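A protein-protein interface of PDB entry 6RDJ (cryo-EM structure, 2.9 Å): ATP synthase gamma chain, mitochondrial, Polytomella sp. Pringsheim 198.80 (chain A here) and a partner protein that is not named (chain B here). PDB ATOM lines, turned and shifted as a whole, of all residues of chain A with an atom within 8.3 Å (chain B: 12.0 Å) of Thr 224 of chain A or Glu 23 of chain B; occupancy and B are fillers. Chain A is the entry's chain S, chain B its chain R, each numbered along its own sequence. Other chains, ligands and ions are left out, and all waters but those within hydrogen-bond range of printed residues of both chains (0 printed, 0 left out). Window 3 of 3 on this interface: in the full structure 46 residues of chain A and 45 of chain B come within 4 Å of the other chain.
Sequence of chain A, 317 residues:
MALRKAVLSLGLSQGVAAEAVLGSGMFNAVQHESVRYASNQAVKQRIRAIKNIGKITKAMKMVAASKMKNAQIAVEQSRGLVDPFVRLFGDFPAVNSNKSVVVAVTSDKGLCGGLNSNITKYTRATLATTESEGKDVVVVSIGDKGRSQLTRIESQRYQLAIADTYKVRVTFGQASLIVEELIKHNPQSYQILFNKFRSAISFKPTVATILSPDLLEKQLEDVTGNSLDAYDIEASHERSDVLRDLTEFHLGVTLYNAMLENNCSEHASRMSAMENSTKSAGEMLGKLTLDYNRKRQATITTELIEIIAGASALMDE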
ATOM      1  N   LEU A 216     -22.321  22.865   6.938  1.00  0.00           N
ATOM      2  CA  LEU A 216     -22.570  21.496   7.360  1.00  0.00           C
ATOM      3  C   LEU A 216     -22.241  20.458   6.301  1.00  0.00           C
ATOM      4  O   LEU A 216     -21.966  19.310   6.661  1.00  0.00           O
ATOM      5  CB  LEU A 216     -24.033  21.354   7.783  1.00  0.00           C
ATOM      6  CG  LEU A 216     -24.509  20.159   8.602  1.00  0.00           C
ATOM      7  CD1 LEU A 216     -23.828  20.152   9.944  1.00  0.00           C
ATOM      8  CD2 LEU A 216     -25.991  20.267   8.786  1.00  0.00           C
ATOM      9  N   LYS A 218     -19.694  20.125   3.926  1.00  0.00           N
ATOM     10  CA  LYS A 218     -18.319  19.647   3.924  1.00  0.00           C
ATOM     11  C   LYS A 218     -17.990  18.920   5.219  1.00  0.00           C
ATOM     12  O   LYS A 218     -17.174  17.995   5.215  1.00  0.00           O
ATOM     13  CB  LYS A 218     -17.372  20.824   3.689  1.00  0.00           C
ATOM     14  CG  LYS A 218     -15.925  20.469   3.380  1.00  0.00           C
ATOM     15  CD  LYS A 218     -15.026  20.563   4.606  1.00  0.00           C
ATOM     16  CE  LYS A 218     -13.587  20.245   4.259  1.00  0.00           C
ATOM     17  NZ  LYS A 218     -12.701  20.311   5.442  1.00  0.00           N
ATOM     18  N   GLN A 219     -18.627  19.306   6.324  1.00  0.00           N
ATOM     19  CA  GLN A 219     -18.398  18.632   7.595  1.00  0.00           C
ATOM     20  C   GLN A 219     -19.027  17.250   7.616  1.00  0.00           C
ATOM     21  O   GLN A 219     -18.521  16.350   8.289  1.00  0.00           O
ATOM     22  CB  GLN A 219     -18.925  19.487   8.739  1.00  0.00           C
ATOM     23  CG  GLN A 219     -18.183  20.796   8.877  1.00  0.00           C
ATOM     24  CD  GLN A 219     -18.620  21.612  10.074  1.00  0.00           C
ATOM     25  OE1 GLN A 219     -19.448  21.175  10.874  1.00  0.00           O
ATOM     26  NE2 GLN A 219     -18.069  22.814  10.200  1.00  0.00           N
ATOM     27  N   LEU A 220     -20.118  17.059   6.889  1.00  0.00           N
ATOM     28  CA  LEU A 220     -20.712  15.738   6.769  1.00  0.00           C
ATOM     29  C   LEU A 220     -20.038  14.875   5.718  1.00  0.00           C
ATOM     30  O   LEU A 220     -20.293  13.667   5.680  1.00  0.00           O
ATOM     31  CB  LEU A 220     -22.202  15.847   6.448  1.00  0.00           C
ATOM     32  CG  LEU A 220     -23.195  15.686   7.602  1.00  0.00           C
ATOM     33  CD1 LEU A 220     -23.111  14.265   8.086  1.00  0.00           C
ATOM     34  CD2 LEU A 220     -22.949  16.647   8.746  1.00  0.00           C
ATOM     35  N   GLU A 221     -19.211  15.451   4.855  1.00  0.00           N
ATOM     36  CA  GLU A 221     -18.528  14.637   3.863  1.00  0.00           C
ATOM     37  C   GLU A 221     -17.152  14.164   4.300  1.00  0.00           C
ATOM     38  O   GLU A 221     -16.640  13.211   3.708  1.00  0.00           O
ATOM     39  CB  GLU A 221     -18.407  15.392   2.545  1.00  0.00           C
ATOM     40  CG  GLU A 221     -19.670  15.356   1.747  1.00  0.00           C
ATOM     41  CD  GLU A 221     -19.778  14.088   0.930  1.00  0.00           C
ATOM     42  OE1 GLU A 221     -18.802  13.741   0.234  1.00  0.00           O
ATOM     43  OE2 GLU A 221     -20.825  13.414   1.007  1.00  0.00           O
ATOM     44  N   ASP A 222     -16.535  14.788   5.299  1.00  0.00           N
ATOM     45  CA  ASP A 222     -15.191  14.361   5.684  1.00  0.00           C
ATOM     46  C   ASP A 222     -15.299  13.154   6.604  1.00  0.00           C
ATOM     47  O   ASP A 222     -15.994  13.162   7.616  1.00  0.00           O
ATOM     48  CB  ASP A 222     -14.360  15.511   6.262  1.00  0.00           C
ATOM     49  CG  ASP A 222     -14.979  16.185   7.464  1.00  0.00           C
ATOM     50  OD1 ASP A 222     -15.039  15.595   8.547  1.00  0.00           O
ATOM     51  OD2 ASP A 222     -15.345  17.365   7.336  1.00  0.00           O
ATOM     52  N   VAL A 223     -14.716  12.048   6.155  1.00  0.00           N
ATOM     53  CA  VAL A 223     -14.524  10.859   6.977  1.00  0.00           C
ATOM     54  C   VAL A 223     -13.023  10.597   6.997  1.00  0.00           C
ATOM     55  O   VAL A 223     -12.499   9.907   6.110  1.00  0.00           O
ATOM     56  CB  VAL A 223     -15.307   9.647   6.454  1.00  0.00           C
ATOM     57  CG1 VAL A 223     -15.153   8.457   7.387  1.00  0.00           C
ATOM     58  CG2 VAL A 223     -16.790   9.990   6.297  1.00  0.00           C
ATOM     59  N   THR A 224     -12.342  11.160   8.004  1.00  0.00           N
ATOM     60  CA  THR A 224     -10.893  11.064   8.231  1.00  0.00           C
ATOM     61  C   THR A 224     -10.115  11.504   6.982  1.00  0.00           C
ATOM     62  O   THR A 224      -9.494  10.709   6.270  1.00  0.00           O
ATOM     63  CB  THR A 224     -10.502   9.654   8.696  1.00  0.00           C
ATOM     64  OG1 THR A 224     -11.399   9.244   9.734  1.00  0.00           O
ATOM     65  CG2 THR A 224      -9.102   9.663   9.297  1.00  0.00           C
ATOM     66  N   GLY A 225     -10.203  12.801   6.704  1.00  0.00           N
ATOM     67  CA  GLY A 225      -9.759  13.351   5.437  1.00  0.00           C
ATOM     68  C   GLY A 225     -10.891  14.101   4.765  1.00  0.00           C
ATOM     69  O   GLY A 225     -11.294  15.154   5.266  1.00  0.00           O
ATOM     70  N   ASN A 226     -11.377  13.582   3.631  1.00  0.00           N
ATOM     71  CA  ASN A 226     -12.661  13.954   3.041  1.00  0.00           C
ATOM     72  C   ASN A 226     -13.036  12.947   1.967  1.00  0.00           C
ATOM     73  O   ASN A 226     -12.191  12.221   1.439  1.00  0.00           O
ATOM     74  CB  ASN A 226     -12.663  15.357   2.428  1.00  0.00           C
ATOM     75  CG  ASN A 226     -14.038  15.984   2.419  1.00  0.00           C
ATOM     76  OD1 ASN A 226     -15.029  15.317   2.142  1.00  0.00           O
ATOM     77  ND2 ASN A 226     -14.105  17.269   2.727  1.00  0.00           N
ATOM     78  N   SER A 227     -14.331  12.910   1.664  1.00  0.00           N
ATOM     79  CA  SER A 227     -14.845  12.275   0.463  1.00  0.00           C
ATOM     80  C   SER A 227     -15.041  13.271  -0.665  1.00  0.00           C
ATOM     81  O   SER A 227     -15.251  12.863  -1.810  1.00  0.00           O
ATOM     82  CB  SER A 227     -16.174  11.580   0.758  1.00  0.00           C
ATOM     83  OG  SER A 227     -17.059  12.469   1.418  1.00  0.00           O
ATOM     84  N   ASP A 229     -12.596  15.682  -1.182  1.00  0.00           N
ATOM     85  CA  ASP A 229     -11.259  16.001  -1.657  1.00  0.00           C
ATOM     86  C   ASP A 229     -10.743  15.018  -2.695  1.00  0.00           C
ATOM     87  O   ASP A 229      -9.596  15.149  -3.127  1.00  0.00           O
ATOM     88  CB  ASP A 229     -10.279  16.087  -0.487  1.00  0.00           C
ATOM     89  CG  ASP A 229     -10.298  17.449   0.184  1.00  0.00           C
ATOM     90  OD1 ASP A 229     -10.536  17.532   1.403  1.00  0.00           O
ATOM     91  OD2 ASP A 229     -10.086  18.458  -0.523  1.00  0.00           O
ATOM     92  N   GLU B  23     -14.980  14.361  13.546  1.00  0.00           N
ATOM     93  CA  GLU B  23     -15.009  15.012  12.242  1.00  0.00           C
ATOM     94  C   GLU B  23     -16.370  14.854  11.560  1.00  0.00           C
ATOM     95  O   GLU B  23     -16.814  15.736  10.824  1.00  0.00           O
ATOM     96  CB  GLU B  23     -13.894  14.460  11.349  1.00  0.00           C
ATOM     97  CG  GLU B  23     -13.744  12.950  11.365  1.00  0.00           C
ATOM     98  CD  GLU B  23     -12.648  12.493  12.308  1.00  0.00           C
ATOM     99  OE1 GLU B  23     -12.098  13.347  13.032  1.00  0.00           O
ATOM    100  OE2 GLU B  23     -12.335  11.283  12.323  1.00  0.00           O
ATOM    101  N   ALA B  24     -17.036  13.734  11.833  1.00  0.00           N
ATOM    102  CA  ALA B  24     -18.336  13.424  11.248  1.00  0.00           C
ATOM    103  C   ALA B  24     -19.368  13.284  12.356  1.00  0.00           C
ATOM    104  O   ALA B  24     -20.116  12.300  12.396  1.00  0.00           O
ATOM    105  CB  ALA B  24     -18.269  12.151  10.405  1.00  0.00           C
ATOM    106  N   ALA B  25     -19.411  14.280  13.254  1.00  0.00           N
ATOM    107  CA  ALA B  25     -20.108  14.223  14.540  1.00  0.00           C
ATOM    108  C   ALA B  25     -21.614  13.997  14.438  1.00  0.00           C
ATOM    109  O   ALA B  25     -22.249  13.723  15.464  1.00  0.00           O
ATOM    110  CB  ALA B  25     -19.842  15.512  15.324  1.00  0.00           C
ATOM    111  N   ALA B  26     -22.205  14.104  13.249  1.00  0.00           N
ATOM    112  CA  ALA B  26     -23.601  13.753  13.023  1.00  0.00           C
ATOM    113  C   ALA B  26     -23.654  12.558  12.080  1.00  0.00           C
ATOM    114  O   ALA B  26     -23.673  12.736  10.856  1.00  0.00           O
ATOM    115  CB  ALA B  26     -24.367  14.942  12.437  1.00  0.00           C
ATOM    116  N   PRO B  27     -23.680  11.320  12.588  1.00  0.00           N
ATOM    117  CA  PRO B  27     -23.750  10.159  11.686  1.00  0.00           C
ATOM    118  C   PRO B  27     -25.108  10.034  11.015  1.00  0.00           C
ATOM    119  O   PRO B  27     -25.949   9.225  11.418  1.00  0.00           O
ATOM    120  CB  PRO B  27     -23.470   8.970  12.612  1.00  0.00           C
ATOM    121  CG  PRO B  27     -22.853   9.563  13.833  1.00  0.00           C
ATOM    122  CD  PRO B  27     -23.457  10.917  13.982  1.00  0.00           C
ATOM    123  N   ALA B  28     -25.315  10.838   9.976  1.00  0.00           N
ATOM    124  CA  ALA B  28     -26.599  10.954   9.305  1.00  0.00           C
ATOM    125  C   ALA B  28     -26.756   9.832   8.289  1.00  0.00           C
ATOM    126  O   ALA B  28     -25.966   8.887   8.234  1.00  0.00           O
ATOM    127  CB  ALA B  28     -26.720  12.319   8.643  1.00  0.00           C
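OD1 of Asp 222 of chain A lies close to O of Glu 23 of chain B (2.9 Å). The side-chain carboxylate of Glu 23 of chain B is in hydrogen-bond range of the side-chain hydroxyl of Thr 224 of chain A (3.4 Å). O of Gln 219 of chain A lies close to O of Glu 23 of chain B, 3.1 Å away.
Leu 220 of chain A touches Ala 26 of chain B (CD1 to O, 3.2 Å). O of Asp 222 of chain A touches CB of Ala 24 of chain B (3.7 Å).
Thr 224 of chain A touches just one residue of chain B: Glu 23 (3.4 Å). Glu 23 of chain B touches just these residues of chain A: Gln 219 (3.1 Å), Asp 222 (2.9 Å) and Thr 224 (3.4 Å). Gln 219 of chain A touches just one residue of chain B: Glu 23 (3.1 Å). Leu 220 of chain A touches one residue of chain B. No residue of chain B comes within 4 Å of Val 223 of chain A. No residue of chain B comes within 4 Å of Gly 225 of chain A. Printed residues of chain A within 4 Å of Ala 24 of chain B: Asp 222 (3.7 Å). Printed residues of chain A within 4 Å of Ala 26 of chain B: Leu 220. Ala 28 of chain B touches none of the printed residues of chain A. Asp 229 of chain A touches none of the printed residues of chain B. The nearest residue of chain B that does not touch Thr 224 of chain A is Ala 24 of chain B (6.5 Å). The nearest residue of chain A that does not touch Glu 23 of chain B is Val 223 of chain A (4.9 Å).
Hydrophobic or aromatic side chains of chain A within 4 Å of the printed part of chain B: Leu 220. Printed residues of chain B that touch a printed residue of chain A: Glu 23, Ala 24 and Ala 26. Hydrophobic or aromatic side chains of chain B that line the printed part of chain A: Ala 24. Along chain B the printed residues that touch a printed residue of chain A span positions 23 to 26.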
